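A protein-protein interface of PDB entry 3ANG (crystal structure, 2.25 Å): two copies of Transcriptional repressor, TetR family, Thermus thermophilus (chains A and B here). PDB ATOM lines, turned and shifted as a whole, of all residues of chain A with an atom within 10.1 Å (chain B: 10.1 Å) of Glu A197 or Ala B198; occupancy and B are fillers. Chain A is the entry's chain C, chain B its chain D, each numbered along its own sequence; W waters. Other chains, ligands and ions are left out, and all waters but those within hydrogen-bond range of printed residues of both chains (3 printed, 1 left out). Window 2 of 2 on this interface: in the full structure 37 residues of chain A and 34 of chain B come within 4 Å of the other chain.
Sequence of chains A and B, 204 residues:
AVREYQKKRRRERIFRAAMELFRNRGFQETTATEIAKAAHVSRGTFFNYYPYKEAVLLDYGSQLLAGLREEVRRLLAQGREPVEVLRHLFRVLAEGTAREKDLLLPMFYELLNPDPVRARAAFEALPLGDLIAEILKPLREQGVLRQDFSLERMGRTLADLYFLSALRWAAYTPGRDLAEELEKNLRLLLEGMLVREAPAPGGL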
ATOM      1  N   GLY A 143      28.297 -39.747 -17.606  1.00  0.00           N
ATOM      2  CA  GLY A 143      26.908 -39.656 -18.026  1.00  0.00           C
ATOM      3  C   GLY A 143      26.453 -38.414 -18.777  1.00  0.00           C
ATOM      4  O   GLY A 143      25.280 -38.323 -19.136  1.00  0.00           O
ATOM      5  N   GLU A 191      28.715 -28.233 -27.236  1.00  0.00           N
ATOM      6  CA  GLU A 191      27.394 -27.787 -26.797  1.00  0.00           C
ATOM      7  C   GLU A 191      26.306 -27.757 -27.855  1.00  0.00           C
ATOM      8  O   GLU A 191      25.124 -27.727 -27.510  1.00  0.00           O
ATOM      9  CB  GLU A 191      27.469 -26.387 -26.199  1.00  0.00           C
ATOM     10  CG  GLU A 191      28.463 -26.174 -25.081  1.00  0.00           C
ATOM     11  CD  GLU A 191      28.533 -24.698 -24.704  1.00  0.00           C
ATOM     12  OE1 GLU A 191      27.663 -24.219 -23.932  1.00  0.00           O
ATOM     13  OE2 GLU A 191      29.443 -24.007 -25.208  1.00  0.00           O
ATOM     14  N   GLY A 192      26.694 -27.737 -29.127  1.00  0.00           N
ATOM     15  CA  GLY A 192      25.707 -27.691 -30.197  1.00  0.00           C
ATOM     16  C   GLY A 192      25.219 -26.263 -30.413  1.00  0.00           C
ATOM     17  O   GLY A 192      25.520 -25.377 -29.604  1.00  0.00           O
ATOM     18  N   LEU A 194      21.934 -25.462 -30.639  1.00  0.00           N
ATOM     19  CA  LEU A 194      20.682 -25.325 -29.903  1.00  0.00           C
ATOM     20  C   LEU A 194      20.980 -24.831 -28.510  1.00  0.00           C
ATOM     21  O   LEU A 194      21.901 -25.328 -27.862  1.00  0.00           O
ATOM     22  CB  LEU A 194      19.964 -26.679 -29.834  1.00  0.00           C
ATOM     23  CG  LEU A 194      19.245 -27.052 -31.129  1.00  0.00           C
ATOM     24  CD1 LEU A 194      18.843 -28.521 -31.125  1.00  0.00           C
ATOM     25  CD2 LEU A 194      18.035 -26.155 -31.272  1.00  0.00           C
ATOM     26  N   VAL A 195      20.202 -23.862 -28.031  1.00  0.00           N
ATOM     27  CA  VAL A 195      20.451 -23.341 -26.691  1.00  0.00           C
ATOM     28  C   VAL A 195      20.288 -24.428 -25.626  1.00  0.00           C
ATOM     29  O   VAL A 195      19.571 -25.425 -25.817  1.00  0.00           O
ATOM     30  CB  VAL A 195      19.535 -22.118 -26.348  1.00  0.00           C
ATOM     31  CG1 VAL A 195      19.798 -20.971 -27.353  1.00  0.00           C
ATOM     32  CG2 VAL A 195      18.062 -22.530 -26.355  1.00  0.00           C
ATOM     33  N   ARG A 196      20.989 -24.233 -24.517  1.00  0.00           N
ATOM     34  CA  ARG A 196      20.950 -25.158 -23.399  1.00  0.00           C
ATOM     35  C   ARG A 196      20.358 -24.494 -22.153  1.00  0.00           C
ATOM     36  O   ARG A 196      20.193 -23.272 -22.099  1.00  0.00           O
ATOM     37  CB  ARG A 196      22.365 -25.671 -23.095  1.00  0.00           C
ATOM     38  CG  ARG A 196      22.838 -26.693 -24.107  1.00  0.00           C
ATOM     39  CD  ARG A 196      24.270 -27.139 -23.898  1.00  0.00           C
ATOM     40  NE  ARG A 196      24.540 -28.210 -24.847  1.00  0.00           N
ATOM     41  CZ  ARG A 196      24.161 -29.470 -24.679  1.00  0.00           C
ATOM     42  NH1 ARG A 196      23.518 -29.833 -23.576  1.00  0.00           N
ATOM     43  NH2 ARG A 196      24.374 -30.357 -25.643  1.00  0.00           N
ATOM     44  N   GLU A 197      20.036 -25.319 -21.165  1.00  0.00           N
ATOM     45  CA  GLU A 197      19.469 -24.843 -19.917  1.00  0.00           C
ATOM     46  C   GLU A 197      20.485 -24.073 -19.076  1.00  0.00           C
ATOM     47  O   GLU A 197      21.591 -24.549 -18.833  1.00  0.00           O
ATOM     48  CB  GLU A 197      18.940 -26.030 -19.106  1.00  0.00           C
ATOM     49  CG  GLU A 197      18.499 -25.656 -17.696  1.00  0.00           C
ATOM     50  CD  GLU A 197      17.942 -26.845 -16.926  1.00  0.00           C
ATOM     51  OE1 GLU A 197      16.911 -27.402 -17.367  1.00  0.00           O
ATOM     52  OE2 GLU A 197      18.536 -27.220 -15.886  1.00  0.00           O
ATOM     53  N   ALA A 198      20.114 -22.871 -18.646  1.00  0.00           N
ATOM     54  CA  ALA A 198      20.985 -22.080 -17.790  1.00  0.00           C
ATOM     55  C   ALA A 198      20.702 -22.577 -16.371  1.00  0.00           C
ATOM     56  O   ALA A 198      19.544 -22.767 -15.997  1.00  0.00           O
ATOM     57  CB  ALA A 198      20.652 -20.600 -17.910  1.00  0.00           C
ATOM     58  N   PRO A 199      21.752 -22.802 -15.562  1.00  0.00           N
ATOM     59  CA  PRO A 199      21.537 -23.283 -14.192  1.00  0.00           C
ATOM     60  C   PRO A 199      20.928 -22.198 -13.315  1.00  0.00           C
ATOM     61  O   PRO A 199      21.031 -21.018 -13.629  1.00  0.00           O
ATOM     62  CB  PRO A 199      22.948 -23.639 -13.703  1.00  0.00           C
ATOM     63  CG  PRO A 199      23.829 -23.560 -14.940  1.00  0.00           C
ATOM     64  CD  PRO A 199      23.177 -22.530 -15.806  1.00  0.00           C
ATOM     65  N   ALA A 200      20.301 -22.597 -12.216  1.00  0.00           N
ATOM     66  CA  ALA A 200      19.736 -21.619 -11.294  1.00  0.00           C
ATOM     67  C   ALA A 200      20.953 -20.852 -10.787  1.00  0.00           C
ATOM     68  O   ALA A 200      21.975 -21.458 -10.468  1.00  0.00           O
ATOM     69  CB  ALA A 200      19.032 -22.323 -10.132  1.00  0.00           C
ATOM     70  N   PRO A 201      20.869 -19.515 -10.718  1.00  0.00           N
ATOM     71  CA  PRO A 201      22.010 -18.727 -10.240  1.00  0.00           C
ATOM     72  C   PRO A 201      22.382 -19.037  -8.796  1.00  0.00           C
ATOM     73  O   PRO A 201      21.560 -19.523  -8.020  1.00  0.00           O
ATOM     74  CB  PRO A 201      21.528 -17.296 -10.416  1.00  0.00           C
ATOM     75  CG  PRO A 201      20.046 -17.424 -10.157  1.00  0.00           C
ATOM     76  CD  PRO A 201      19.699 -18.652 -10.957  1.00  0.00           C
ATOM     77  N   VAL B 144      15.678 -20.326 -30.658  1.00  0.00           N
ATOM     78  CA  VAL B 144      16.307 -21.526 -30.101  1.00  0.00           C
ATOM     79  C   VAL B 144      17.796 -21.778 -30.404  1.00  0.00           C
ATOM     80  O   VAL B 144      18.332 -22.828 -30.035  1.00  0.00           O
ATOM     81  CB  VAL B 144      15.515 -22.778 -30.490  1.00  0.00           C
ATOM     82  CG1 VAL B 144      14.055 -22.602 -30.086  1.00  0.00           C
ATOM     83  CG2 VAL B 144      15.616 -23.020 -31.978  1.00  0.00           C
ATOM     84  N   ARG B 146      21.901 -20.479 -30.112  1.00  0.00           N
ATOM     85  CA  ARG B 146      22.731 -19.598 -29.311  1.00  0.00           C
ATOM     86  C   ARG B 146      23.036 -18.327 -30.122  1.00  0.00           C
ATOM     87  O   ARG B 146      22.996 -18.334 -31.360  1.00  0.00           O
ATOM     88  CB  ARG B 146      24.026 -20.300 -28.902  1.00  0.00           C
ATOM     89  CG  ARG B 146      24.879 -20.769 -30.076  1.00  0.00           C
ATOM     90  CD  ARG B 146      26.313 -20.983 -29.637  1.00  0.00           C
ATOM     91  NE  ARG B 146      26.516 -22.294 -29.073  1.00  0.00           N
ATOM     92  CZ  ARG B 146      27.425 -22.581 -28.151  1.00  0.00           C
ATOM     93  NH1 ARG B 146      28.228 -21.633 -27.664  1.00  0.00           N
ATOM     94  NH2 ARG B 146      27.549 -23.834 -27.739  1.00  0.00           N
ATOM     95  N   GLU B 191      23.020 -30.432 -32.074  1.00  0.00           N
ATOM     96  CA  GLU B 191      22.765 -30.842 -30.704  1.00  0.00           C
ATOM     97  C   GLU B 191      23.947 -30.838 -29.748  1.00  0.00           C
ATOM     98  O   GLU B 191      23.756 -30.724 -28.539  1.00  0.00           O
ATOM     99  CB  GLU B 191      22.141 -32.240 -30.715  1.00  0.00           C
ATOM    100  CG  GLU B 191      20.922 -32.365 -31.634  1.00  0.00           C
ATOM    101  CD  GLU B 191      20.541 -33.813 -31.927  1.00  0.00           C
ATOM    102  OE1 GLU B 191      19.588 -34.027 -32.704  1.00  0.00           O
ATOM    103  OE2 GLU B 191      21.187 -34.735 -31.390  1.00  0.00           O
ATOM    104  N   LEU B 194      27.413 -33.166 -25.648  1.00  0.00           N
ATOM    105  CA  LEU B 194      26.845 -33.263 -24.304  1.00  0.00           C
ATOM    106  C   LEU B 194      25.363 -33.608 -24.450  1.00  0.00           C
ATOM    107  O   LEU B 194      24.684 -33.061 -25.313  1.00  0.00           O
ATOM    108  CB  LEU B 194      27.002 -31.928 -23.579  1.00  0.00           C
ATOM    109  CG  LEU B 194      28.439 -31.512 -23.234  1.00  0.00           C
ATOM    110  CD1 LEU B 194      28.455 -30.093 -22.691  1.00  0.00           C
ATOM    111  CD2 LEU B 194      29.024 -32.476 -22.202  1.00  0.00           C
ATOM    112  N   VAL B 195      24.855 -34.515 -23.619  1.00  0.00           N
ATOM    113  CA  VAL B 195      23.448 -34.904 -23.722  1.00  0.00           C
ATOM    114  C   VAL B 195      22.448 -33.760 -23.448  1.00  0.00           C
ATOM    115  O   VAL B 195      22.798 -32.733 -22.862  1.00  0.00           O
ATOM    116  CB  VAL B 195      23.120 -36.071 -22.756  1.00  0.00           C
ATOM    117  CG1 VAL B 195      24.032 -37.276 -23.041  1.00  0.00           C
ATOM    118  CG2 VAL B 195      23.275 -35.607 -21.317  1.00  0.00           C
ATOM    119  N   ARG B 196      21.213 -33.951 -23.914  1.00  0.00           N
ATOM    120  CA  ARG B 196      20.109 -33.007 -23.700  1.00  0.00           C
ATOM    121  C   ARG B 196      19.038 -33.801 -22.963  1.00  0.00           C
ATOM    122  O   ARG B 196      18.178 -34.406 -23.594  1.00  0.00           O
ATOM    123  CB  ARG B 196      19.564 -32.490 -25.039  1.00  0.00           C
ATOM    124  CG  ARG B 196      20.469 -31.413 -25.634  1.00  0.00           C
ATOM    125  CD  ARG B 196      20.197 -31.071 -27.092  1.00  0.00           C
ATOM    126  NE  ARG B 196      21.180 -30.078 -27.509  1.00  0.00           N
ATOM    127  CZ  ARG B 196      21.120 -28.788 -27.202  1.00  0.00           C
ATOM    128  NH1 ARG B 196      20.104 -28.311 -26.487  1.00  0.00           N
ATOM    129  NH2 ARG B 196      22.100 -27.981 -27.565  1.00  0.00           N
ATOM    130  N   GLU B 197      19.096 -33.802 -21.633  1.00  0.00           N
ATOM    131  CA  GLU B 197      18.140 -34.587 -20.839  1.00  0.00           C
ATOM    132  C   GLU B 197      17.397 -33.805 -19.754  1.00  0.00           C
ATOM    133  O   GLU B 197      17.011 -34.371 -18.725  1.00  0.00           O
ATOM    134  CB  GLU B 197      18.862 -35.778 -20.182  1.00  0.00           C
ATOM    135  CG  GLU B 197      19.584 -36.703 -21.171  1.00  0.00           C
ATOM    136  CD  GLU B 197      20.435 -37.769 -20.490  1.00  0.00           C
ATOM    137  OE1 GLU B 197      20.861 -38.702 -21.196  1.00  0.00           O
ATOM    138  OE2 GLU B 197      20.687 -37.679 -19.261  1.00  0.00           O
ATOM    139  N   ALA B 198      17.200 -32.512 -19.980  1.00  0.00           N
ATOM    140  CA  ALA B 198      16.498 -31.679 -19.021  1.00  0.00           C
ATOM    141  C   ALA B 198      15.108 -32.235 -18.761  1.00  0.00           C
ATOM    142  O   ALA B 198      14.380 -32.554 -19.690  1.00  0.00           O
ATOM    143  CB  ALA B 198      16.384 -30.239 -19.545  1.00  0.00           C
ATOM    144  N   PRO B 199      14.740 -32.399 -17.487  1.00  0.00           N
ATOM    145  CA  PRO B 199      13.397 -32.915 -17.219  1.00  0.00           C
ATOM    146  C   PRO B 199      12.368 -31.896 -17.739  1.00  0.00           C
ATOM    147  O   PRO B 199      11.252 -32.260 -18.088  1.00  0.00           O
ATOM    148  CB  PRO B 199      13.369 -33.030 -15.696  1.00  0.00           C
ATOM    149  CG  PRO B 199      14.795 -33.382 -15.372  1.00  0.00           C
ATOM    150  CD  PRO B 199      15.584 -32.462 -16.281  1.00  0.00           C
ATOM    151  N   ALA B 200      12.761 -30.628 -17.817  1.00  0.00           N
ATOM    152  CA  ALA B 200      11.844 -29.577 -18.282  1.00  0.00           C
ATOM    153  C   ALA B 200      12.425 -28.659 -19.357  1.00  0.00           C
ATOM    154  O   ALA B 200      12.826 -27.518 -19.072  1.00  0.00           O
ATOM    155  CB  ALA B 200      11.377 -28.751 -17.093  1.00  0.00           C
ATOM    156  N   PRO B 201      12.454 -29.137 -20.610  1.00  0.00           N
ATOM    157  CA  PRO B 201      12.982 -28.379 -21.756  1.00  0.00           C
ATOM    158  C   PRO B 201      12.123 -27.149 -22.021  1.00  0.00           C
ATOM    159  O   PRO B 201      10.971 -27.083 -21.601  1.00  0.00           O
ATOM    160  CB  PRO B 201      12.882 -29.363 -22.929  1.00  0.00           C
ATOM    161  CG  PRO B 201      12.698 -30.735 -22.267  1.00  0.00           C
ATOM    162  CD  PRO B 201      11.859 -30.410 -21.050  1.00  0.00           C
ATOM    163  N   GLY B 202      12.691 -26.187 -22.736  1.00  0.00           N
ATOM    164  CA  GLY B 202      11.953 -24.987 -23.062  1.00  0.00           C
ATOM    165  C   GLY B 202      10.929 -25.302 -24.129  1.00  0.00           C
ATOM    166  O   GLY B 202      10.780 -26.465 -24.540  1.00  0.00           O
ATOM    167  N   GLY B 203      10.229 -24.266 -24.585  1.00  0.00           N
ATOM    168  CA  GLY B 203       9.213 -24.454 -25.600  1.00  0.00           C
ATOM    169  C   GLY B 203       7.943 -24.958 -24.951  1.00  0.00           C
ATOM    170  O   GLY B 203       7.468 -26.054 -25.331  1.00  0.00           O
HETATM  171  O   HOH W   1      15.683 -26.742 -19.427  1.00  0.00           O
HETATM  172  O   HOH W   2      22.788 -38.195 -17.479  1.00  0.00           O
HETATM  173  O   HOH W   3      14.875 -29.356 -16.578  1.00  0.00           O
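Glu A191 touches its own counterpart, Glu B191. Glu A191 touches Arg B196, and with the chains exchanged Arg A196 touches Glu B191. Leu A194 touches Arg B196, and with the chains exchanged Arg A196 touches Leu B194. Arg B196 touches its own counterpart, Arg A196.
Of the 11 printed residues of chain A, 6 touch a printed residue of chain B. Printed residues of chain A that touch a printed residue of chain B: Glu A191, Gly A192, Leu A194, Val A195, Arg A196 and Glu A197. Hydrophobic or aromatic side chains of chain A that line the printed part of chain B: Leu A194 and Val A195. Of the 13 printed residues of chain B, 7 touch a printed residue of chain A. Printed residues of chain B that touch a printed residue of chain A: Val B144, Arg B146, Glu B191, Leu B194, Val B195, Arg B196 and Ala B198. Hydrophobic or aromatic side chains of chain B that line the printed part of chain A: Leu B194 and Ala B198.
OE2 of Glu A191 is in salt-bridge range of NH2 of Arg B146 (3.2 Å). The guanidinium group (NH2) of Arg B196 sits at hydrogen-bond distance from the backbone carbonyl oxygen (O) of Glu A191. The backbone carbonyl oxygen (O) of Gly A192 sits at hydrogen-bond distance from the guanidinium group (NH2) of Arg B146, at 3.2 Å. The guanidinium group (NH2) of Arg B196 lies within hydrogen-bond range of the backbone carbonyl oxygen (O) of Leu A194. The backbone NH (N) of Val A195 sits at hydrogen-bond distance from the backbone carbonyl oxygen (O) of Val B144 (2.9 Å). O of Val A195 is in hydrogen-bond range of NH1 of Arg B196, at 3.0 Å. NH2 of Arg A196 lies within hydrogen-bond range of O of Glu B191 (3.0 Å). The guanidinium group of Arg A196 sits at hydrogen-bond distance from the backbone carbonyl oxygen of Leu B194 (2.7 Å). The guanidinium group (NH1) of Arg A196 sits at hydrogen-bond distance from the backbone carbonyl oxygen (O) of Val B195 (3.1 Å). O of Glu B191 lies close to O of Glu A191 (3.5 Å).
Of the printed residues of chain B, Glu A197 touches Ala B198 (3.6 Å). Ala B198 touches just one residue of chain A: Glu A197 (3.6 Å). No residue of chain A comes within 4 Å of Pro B199. No residue of chain A comes within 4 Å of Ala B200. Of the printed residues of chain B, Arg A196 touches Glu B191 (3.0 Å), Leu B194 (2.7 Å), Val B195 (3.1 Å) and Arg B196 (3.7 Å). Of the printed residues of chain B, Val A195 touches Val B144, Arg B146 and Arg B196. Of the printed residues of chain A, Arg B146 touches Glu A191, Gly A192 and Val A195. Gly A143 touches none of the printed residues of chain B. The nearest residue of chain B that does not touch Glu A197 is Ala B200 (4.4 Å). The nearest printed residue of chain A that does not touch Val B144 is Arg A196 (6.3 Å).
NE of Arg A196 lies within hydrogen-bond range of O of Glu A191 (2.8 Å). O of Glu B191 lies within hydrogen-bond range of NE of Arg B196.
Water W1 lies within hydrogen-bond range of the side-chain carboxylate (OE1) of Glu A197 (2.5 Å) and the backbone carbonyl oxygen (O) of Ala B200 (3.0 Å). Water W3 lies within hydrogen-bond range of the backbone NH (N) of Ala B200 (2.8 Å) and the side-chain carboxylate (OE1) of Glu A197 (2.9 Å). Water W2 lies within hydrogen-bond range of OE2 of Glu B197 (2.8 Å) and O of Gly A143 (3.0 Å).
Glu B191 touches Gly A192. Val B144 touches Leu A194 (O to CA, 3.4 Å). N of Arg B146 touches CG1 of Val A195, 3.5 Å away. NH2 of Arg B196 touches NE of Arg A196 (3.7 Å). CB of Ala B198 touches OE1 of Glu A197 (3.6 Å).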
